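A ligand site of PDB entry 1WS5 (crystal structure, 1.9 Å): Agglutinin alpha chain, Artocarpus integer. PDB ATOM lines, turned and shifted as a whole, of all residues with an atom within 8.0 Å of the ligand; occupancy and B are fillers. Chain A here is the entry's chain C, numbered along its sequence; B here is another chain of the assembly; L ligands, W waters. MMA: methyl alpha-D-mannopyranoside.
O6 of the ligand sits at hydrogen-bond distance from OD1 of Asp 125 (2.8 Å).
The backbone NH (N) of Gly 1 is in hydrogen-bond range of an oxygen (O3) of the ligand, at 2.8 Å.
N of Trp 123 sits at hydrogen-bond distance from O6 of the ligand, at 2.9 Å.
An oxygen (O6) of the ligand is in hydrogen-bond range of the backbone carbonyl oxygen (O) of Trp 123, 3.0 Å away.
N of Tyr 122 is in hydrogen-bond range of O6 of the ligand, 2.9 Å away.
O6 of the ligand lies close to N of Gly 121 (3.5 Å).
OD2 of Asp 125 is in hydrogen-bond range of N of Gly 1 (3.5 Å).
N of Gly 121 is in hydrogen-bond range of OD2 of Asp 125 (3.4 Å).
The backbone carbonyl oxygen of Ser 119 is in hydrogen-bond range of the backbone NH of Asp 125 (2.8 Å).
The backbone NH (N) of Ala 17 of chain B lies within hydrogen-bond range of the backbone carbonyl oxygen (O) of Asp 125, 2.9 Å away.
OG of Ser 46 lies within hydrogen-bond range of O of Tyr 122, 2.6 Å away.
N of Phe 47 lies within hydrogen-bond range of O of Gly 121, 3.0 Å away.
Phe 47 touches the ligand (CE2 to O2, 3.3 Å).
Tyr 78 touches the ligand.
Hydrophobic or aromatic side chains within 4 Å of the ligand: Phe 47, Tyr 78, Tyr 122 and Trp 123.
Within 4 Å of the ligand: Gly 1, Phe 47, Tyr 78, Gly 121, Tyr 122, Trp 123 and Asp 125.
The nearest printed residue that does not touch the ligand is Val 80 (4.02 Å).
Water W2 bridges the backbone NH (N) of Gly 1 (2.8 Å) and an oxygen (O3) of the ligand (3.3 Å).
Water W3 lies within hydrogen-bond range of the backbone carbonyl oxygen of Val 79 (2.9 Å), the side-chain carboxylate of Asp 125 (3.1 Å) and an oxygen (O4) of the ligand (3.5 Å).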
ATOM      1  N   GLY A   1      31.233  -2.677  -8.818  1.00  0.00           N
ATOM      2  CA  GLY A   1      31.240  -4.121  -9.146  1.00  0.00           C
ATOM      3  C   GLY A   1      32.656  -4.668  -9.208  1.00  0.00           C
ATOM      4  O   GLY A   1      33.608  -4.019  -8.784  1.00  0.00           O
ATOM      5  N   LYS A   2      32.783  -5.880  -9.758  1.00  0.00           N
ATOM      6  CA  LYS A   2      34.073  -6.546  -9.883  1.00  0.00           C
ATOM      7  C   LYS A   2      34.780  -6.130 -11.172  1.00  0.00           C
ATOM      8  O   LYS A   2      34.279  -6.397 -12.270  1.00  0.00           O
ATOM      9  CB  LYS A   2      33.857  -8.059  -9.879  1.00  0.00           C
ATOM     10  CG  LYS A   2      35.122  -8.880  -9.701  1.00  0.00           C
ATOM     11  CD  LYS A   2      34.794 -10.369  -9.741  1.00  0.00           C
ATOM     12  CE  LYS A   2      35.931 -11.215  -9.167  1.00  0.00           C
ATOM     13  NZ  LYS A   2      37.239 -10.935  -9.827  1.00  0.00           N
ATOM     14  N   ALA A  24      19.815  -3.718 -18.188  1.00  0.00           N
ATOM     15  CA  ALA A  24      21.058  -3.424 -18.888  1.00  0.00           C
ATOM     16  C   ALA A  24      21.811  -4.684 -19.245  1.00  0.00           C
ATOM     17  O   ALA A  24      21.291  -5.790 -19.124  1.00  0.00           O
ATOM     18  CB  ALA A  24      21.924  -2.534 -18.001  1.00  0.00           C
ATOM     19  N   ILE A  25      23.060  -4.502 -19.682  1.00  0.00           N
ATOM     20  CA  ILE A  25      23.909  -5.618 -20.056  1.00  0.00           C
ATOM     21  C   ILE A  25      24.433  -6.307 -18.809  1.00  0.00           C
ATOM     22  O   ILE A  25      24.796  -5.646 -17.835  1.00  0.00           O
ATOM     23  CB  ILE A  25      25.065  -5.126 -20.931  1.00  0.00           C
ATOM     24  CG1 ILE A  25      24.495  -4.681 -22.278  1.00  0.00           C
ATOM     25  CG2 ILE A  25      26.126  -6.217 -21.101  1.00  0.00           C
ATOM     26  CD1 ILE A  25      25.416  -3.824 -23.048  1.00  0.00           C
ATOM     27  N   GLY A  26      24.446  -7.638 -18.838  1.00  0.00           N
ATOM     28  CA  GLY A  26      24.919  -8.390 -17.693  1.00  0.00           C
ATOM     29  C   GLY A  26      26.294  -9.029 -17.868  1.00  0.00           C
ATOM     30  O   GLY A  26      27.303  -8.420 -17.529  1.00  0.00           O
ATOM     31  N   SER A  46      27.568 -11.313 -14.217  1.00  0.00           N
ATOM     32  CA  SER A  46      26.790 -10.443 -13.350  1.00  0.00           C
ATOM     33  C   SER A  46      26.531 -11.202 -12.041  1.00  0.00           C
ATOM     34  O   SER A  46      26.550 -12.433 -12.019  1.00  0.00           O
ATOM     35  CB  SER A  46      25.456 -10.114 -14.014  1.00  0.00           C
ATOM     36  OG  SER A  46      24.505  -9.699 -13.038  1.00  0.00           O
ATOM     37  N   PHE A  47      26.281 -10.457 -10.963  1.00  0.00           N
ATOM     38  CA  PHE A  47      25.987 -11.062  -9.670  1.00  0.00           C
ATOM     39  C   PHE A  47      24.586 -11.674  -9.638  1.00  0.00           C
ATOM     40  O   PHE A  47      24.290 -12.534  -8.801  1.00  0.00           O
ATOM     41  CB  PHE A  47      26.089 -10.020  -8.549  1.00  0.00           C
ATOM     42  CG  PHE A  47      27.458  -9.408  -8.393  1.00  0.00           C
ATOM     43  CD1 PHE A  47      28.590 -10.057  -8.869  1.00  0.00           C
ATOM     44  CD2 PHE A  47      27.615  -8.206  -7.709  1.00  0.00           C
ATOM     45  CE1 PHE A  47      29.868  -9.510  -8.667  1.00  0.00           C
ATOM     46  CE2 PHE A  47      28.880  -7.654  -7.502  1.00  0.00           C
ATOM     47  CZ  PHE A  47      30.001  -8.309  -7.984  1.00  0.00           C
ATOM     48  N   ILE A  48      23.720 -11.233 -10.545  1.00  0.00           N
ATOM     49  CA  ILE A  48      22.360 -11.762 -10.562  1.00  0.00           C
ATOM     50  C   ILE A  48      22.059 -12.531 -11.843  1.00  0.00           C
ATOM     51  O   ILE A  48      22.884 -12.588 -12.759  1.00  0.00           O
ATOM     52  CB  ILE A  48      21.310 -10.654 -10.399  1.00  0.00           C
ATOM     53  CG1 ILE A  48      21.423  -9.648 -11.538  1.00  0.00           C
ATOM     54  CG2 ILE A  48      21.505  -9.970  -9.051  1.00  0.00           C
ATOM     55  CD1 ILE A  48      20.316  -8.610 -11.548  1.00  0.00           C
ATOM     56  N   VAL A  75      20.197   2.876 -13.791  1.00  0.00           N
ATOM     57  CA  VAL A  75      19.384   1.701 -13.506  1.00  0.00           C
ATOM     58  C   VAL A  75      19.448   1.505 -12.001  1.00  0.00           C
ATOM     59  O   VAL A  75      20.524   1.220 -11.453  1.00  0.00           O
ATOM     60  CB  VAL A  75      19.915   0.435 -14.218  1.00  0.00           C
ATOM     61  CG1 VAL A  75      19.093  -0.780 -13.793  1.00  0.00           C
ATOM     62  CG2 VAL A  75      19.835   0.611 -15.725  1.00  0.00           C
ATOM     63  N   SER A  76      18.319   1.671 -11.321  1.00  0.00           N
ATOM     64  CA  SER A  76      18.259   1.516  -9.867  1.00  0.00           C
ATOM     65  C   SER A  76      19.319   2.356  -9.154  1.00  0.00           C
ATOM     66  O   SER A  76      19.901   1.915  -8.160  1.00  0.00           O
ATOM     67  CB  SER A  76      18.432   0.050  -9.476  1.00  0.00           C
ATOM     68  OG  SER A  76      17.364  -0.733  -9.987  1.00  0.00           O
ATOM     69  N   GLY A  77      19.575   3.552  -9.678  1.00  0.00           N
ATOM     70  CA  GLY A  77      20.548   4.434  -9.065  1.00  0.00           C
ATOM     71  C   GLY A  77      21.981   4.333  -9.563  1.00  0.00           C
ATOM     72  O   GLY A  77      22.825   5.134  -9.180  1.00  0.00           O
ATOM     73  N   TYR A  78      22.258   3.356 -10.425  1.00  0.00           N
ATOM     74  CA  TYR A  78      23.613   3.193 -10.949  1.00  0.00           C
ATOM     75  C   TYR A  78      23.705   3.504 -12.436  1.00  0.00           C
ATOM     76  O   TYR A  78      22.816   3.125 -13.205  1.00  0.00           O
ATOM     77  CB  TYR A  78      24.095   1.759 -10.735  1.00  0.00           C
ATOM     78  CG  TYR A  78      24.083   1.313  -9.296  1.00  0.00           C
ATOM     79  CD1 TYR A  78      25.138   1.636  -8.436  1.00  0.00           C
ATOM     80  CD2 TYR A  78      23.034   0.560  -8.792  1.00  0.00           C
ATOM     81  CE1 TYR A  78      25.134   1.215  -7.102  1.00  0.00           C
ATOM     82  CE2 TYR A  78      23.014   0.143  -7.463  1.00  0.00           C
ATOM     83  CZ  TYR A  78      24.068   0.468  -6.625  1.00  0.00           C
ATOM     84  OH  TYR A  78      24.041   0.048  -5.314  1.00  0.00           O
ATOM     85  N   VAL A  79      24.752   4.200 -12.833  1.00  0.00           N
ATOM     86  CA  VAL A  79      24.964   4.522 -14.241  1.00  0.00           C
ATOM     87  C   VAL A  79      25.689   3.302 -14.811  1.00  0.00           C
ATOM     88  O   VAL A  79      26.810   2.996 -14.399  1.00  0.00           O
ATOM     89  CB  VAL A  79      25.835   5.775 -14.419  1.00  0.00           C
ATOM     90  CG1 VAL A  79      26.090   6.025 -15.901  1.00  0.00           C
ATOM     91  CG2 VAL A  79      25.139   6.962 -13.803  1.00  0.00           C
ATOM     92  N   VAL A  80      25.048   2.627 -15.755  1.00  0.00           N
ATOM     93  CA  VAL A  80      25.629   1.435 -16.355  1.00  0.00           C
ATOM     94  C   VAL A  80      25.464   1.429 -17.868  1.00  0.00           C
ATOM     95  O   VAL A  80      24.819   2.321 -18.436  1.00  0.00           O
ATOM     96  CB  VAL A  80      24.948   0.157 -15.795  1.00  0.00           C
ATOM     97  CG1 VAL A  80      25.212   0.045 -14.297  1.00  0.00           C
ATOM     98  CG2 VAL A  80      23.452   0.215 -16.061  1.00  0.00           C
ATOM     99  N   VAL A  81      26.058   0.430 -18.521  1.00  0.00           N
ATOM    100  CA  VAL A  81      25.957   0.283 -19.967  1.00  0.00           C
ATOM    101  C   VAL A  81      24.674  -0.480 -20.204  1.00  0.00           C
ATOM    102  O   VAL A  81      24.577  -1.665 -19.878  1.00  0.00           O
ATOM    103  CB  VAL A  81      27.142  -0.512 -20.533  1.00  0.00           C
ATOM    104  CG1 VAL A  81      26.976  -0.701 -22.033  1.00  0.00           C
ATOM    105  CG2 VAL A  81      28.447   0.211 -20.223  1.00  0.00           C
ATOM    106  N   SER A 119      34.111  -3.262 -15.687  1.00  0.00           N
ATOM    107  CA  SER A 119      33.637  -3.692 -14.374  1.00  0.00           C
ATOM    108  C   SER A 119      32.196  -4.144 -14.466  1.00  0.00           C
ATOM    109  O   SER A 119      31.394  -3.549 -15.190  1.00  0.00           O
ATOM    110  CB  SER A 119      33.760  -2.549 -13.373  1.00  0.00           C
ATOM    111  OG  SER A 119      33.148  -2.897 -12.144  1.00  0.00           O
ATOM    112  N   ILE A 120      31.857  -5.198 -13.739  1.00  0.00           N
ATOM    113  CA  ILE A 120      30.512  -5.721 -13.742  1.00  0.00           C
ATOM    114  C   ILE A 120      30.064  -6.056 -12.321  1.00  0.00           C
ATOM    115  O   ILE A 120      30.773  -6.746 -11.589  1.00  0.00           O
ATOM    116  CB  ILE A 120      30.392  -7.002 -14.595  1.00  0.00           C
ATOM    117  CG1 ILE A 120      30.720  -6.692 -16.061  1.00  0.00           C
ATOM    118  CG2 ILE A 120      28.991  -7.589 -14.457  1.00  0.00           C
ATOM    119  CD1 ILE A 120      30.699  -7.904 -16.964  1.00  0.00           C
ATOM    120  N   GLY A 121      28.901  -5.540 -11.935  1.00  0.00           N
ATOM    121  CA  GLY A 121      28.324  -5.820 -10.631  1.00  0.00           C
ATOM    122  C   GLY A 121      27.048  -6.521 -11.010  1.00  0.00           C
ATOM    123  O   GLY A 121      27.082  -7.651 -11.500  1.00  0.00           O
ATOM    124  N   TYR A 122      25.905  -5.877 -10.791  1.00  0.00           N
ATOM    125  CA  TYR A 122      24.642  -6.464 -11.213  1.00  0.00           C
ATOM    126  C   TYR A 122      24.631  -6.330 -12.732  1.00  0.00           C
ATOM    127  O   TYR A 122      24.117  -7.197 -13.441  1.00  0.00           O
ATOM    128  CB  TYR A 122      23.450  -5.684 -10.652  1.00  0.00           C
ATOM    129  CG  TYR A 122      23.017  -6.122  -9.268  1.00  0.00           C
ATOM    130  CD1 TYR A 122      21.768  -5.753  -8.772  1.00  0.00           C
ATOM    131  CD2 TYR A 122      23.847  -6.914  -8.464  1.00  0.00           C
ATOM    132  CE1 TYR A 122      21.356  -6.169  -7.498  1.00  0.00           C
ATOM    133  CE2 TYR A 122      23.443  -7.325  -7.193  1.00  0.00           C
ATOM    134  CZ  TYR A 122      22.194  -6.954  -6.719  1.00  0.00           C
ATOM    135  OH  TYR A 122      21.778  -7.369  -5.476  1.00  0.00           O
ATOM    136  N   TRP A 123      25.221  -5.244 -13.218  1.00  0.00           N
ATOM    137  CA  TRP A 123      25.297  -4.969 -14.651  1.00  0.00           C
ATOM    138  C   TRP A 123      26.678  -4.448 -15.034  1.00  0.00           C
ATOM    139  O   TRP A 123      27.522  -4.228 -14.160  1.00  0.00           O
ATOM    140  CB  TRP A 123      24.250  -3.922 -15.037  1.00  0.00           C
ATOM    141  CG  TRP A 123      22.880  -4.315 -14.610  1.00  0.00           C
ATOM    142  CD1 TRP A 123      22.113  -5.323 -15.129  1.00  0.00           C
ATOM    143  CD2 TRP A 123      22.144  -3.787 -13.497  1.00  0.00           C
ATOM    144  NE1 TRP A 123      20.949  -5.452 -14.408  1.00  0.00           N
ATOM    145  CE2 TRP A 123      20.946  -4.524 -13.403  1.00  0.00           C
ATOM    146  CE3 TRP A 123      22.385  -2.753 -12.587  1.00  0.00           C
ATOM    147  CZ2 TRP A 123      19.988  -4.261 -12.414  1.00  0.00           C
ATOM    148  CZ3 TRP A 123      21.432  -2.499 -11.599  1.00  0.00           C
ATOM    149  CH2 TRP A 123      20.244  -3.252 -11.528  1.00  0.00           C
ATOM    150  N   LEU A 124      26.897  -4.258 -16.329  1.00  0.00           N
ATOM    151  CA  LEU A 124      28.178  -3.746 -16.823  1.00  0.00           C
ATOM    152  C   LEU A 124      28.279  -2.260 -16.458  1.00  0.00           C
ATOM    153  O   LEU A 124      27.609  -1.414 -17.052  1.00  0.00           O
ATOM    154  CB  LEU A 124      28.262  -3.926 -18.340  1.00  0.00           C
ATOM    155  CG  LEU A 124      29.493  -3.386 -19.057  1.00  0.00           C
ATOM    156  CD1 LEU A 124      30.760  -4.087 -18.556  1.00  0.00           C
ATOM    157  CD2 LEU A 124      29.327  -3.575 -20.556  1.00  0.00           C
ATOM    158  N   ASP A 125      29.127  -1.956 -15.476  1.00  0.00           N
ATOM    159  CA  ASP A 125      29.315  -0.593 -15.001  1.00  0.00           C
ATOM    160  C   ASP A 125      29.967   0.325 -16.015  1.00  0.00           C
ATOM    161  O   ASP A 125      29.533   1.455 -16.233  1.00  0.00           O
ATOM    162  CB  ASP A 125      30.145  -0.600 -13.709  1.00  0.00           C
ATOM    163  CG  ASP A 125      29.534  -1.478 -12.641  1.00  0.00           C
ATOM    164  OD1 ASP A 125      28.346  -1.244 -12.306  1.00  0.00           O
ATOM    165  OD2 ASP A 125      30.221  -2.387 -12.133  1.00  0.00           O
ATOM    166  N   TYR A 126      31.042  -0.161 -16.620  1.00  0.00           N
ATOM    167  CA  TYR A 126      31.765   0.611 -17.612  1.00  0.00           C
ATOM    168  C   TYR A 126      32.726  -0.300 -18.332  1.00  0.00           C
ATOM    169  O   TYR A 126      32.992  -1.427 -17.892  1.00  0.00           O
ATOM    170  CB  TYR A 126      32.536   1.755 -16.948  1.00  0.00           C
ATOM    171  CG  TYR A 126      33.573   1.294 -15.946  1.00  0.00           C
ATOM    172  CD1 TYR A 126      34.809   0.797 -16.365  1.00  0.00           C
ATOM    173  CD2 TYR A 126      33.321   1.340 -14.570  1.00  0.00           C
ATOM    174  CE1 TYR A 126      35.761   0.344 -15.449  1.00  0.00           C
ATOM    175  CE2 TYR A 126      34.261   0.892 -13.649  1.00  0.00           C
ATOM    176  CZ  TYR A 126      35.480   0.400 -14.095  1.00  0.00           C
ATOM    177  OH  TYR A 126      36.415  -0.040 -13.173  1.00  0.00           O
ATOM    178  N   ALA B  17      29.732   4.319 -16.066  1.00  0.00           N
ATOM    179  CA  ALA B  17      29.938   5.029 -14.815  1.00  0.00           C
ATOM    180  C   ALA B  17      31.352   5.604 -14.739  1.00  0.00           C
ATOM    181  O   ALA B  17      32.273   5.121 -15.399  1.00  0.00           O
ATOM    182  CB  ALA B  17      29.706   4.092 -13.635  1.00  0.00           C
HETATM  183  C1  MMA L   1      25.806  -3.741  -7.524  1.00  0.00           C
HETATM  184  C2  MMA L   1      27.285  -3.457  -7.120  1.00  0.00           C
HETATM  185  C3  MMA L   1      27.710  -2.051  -7.590  1.00  0.00           C
HETATM  186  C4  MMA L   1      27.527  -1.918  -9.103  1.00  0.00           C
HETATM  187  C5  MMA L   1      26.057  -2.169  -9.449  1.00  0.00           C
HETATM  188  C6  MMA L   1      25.824  -2.086 -10.945  1.00  0.00           C
HETATM  189  C7  MMA L   1      23.589  -3.133  -6.086  1.00  0.00           C
HETATM  190  O1  MMA L   1      24.962  -3.125  -6.629  1.00  0.00           O
HETATM  191  O2  MMA L   1      28.162  -4.443  -7.642  1.00  0.00           O
HETATM  192  O3  MMA L   1      29.059  -1.821  -7.234  1.00  0.00           O
HETATM  193  O4  MMA L   1      27.926  -0.621  -9.526  1.00  0.00           O
HETATM  194  O5  MMA L   1      25.677  -3.515  -8.995  1.00  0.00           O
HETATM  195  O6  MMA L   1      26.396  -3.172 -11.643  1.00  0.00           O
HETATM  196  O   HOH W   1      30.811  -4.778  -5.846  1.00  0.00           O
HETATM  197  O   HOH W   2      32.150  -2.547  -6.172  1.00  0.00           O
HETATM  198  O   HOH W   3      27.777   1.789 -11.994  1.00  0.00           O
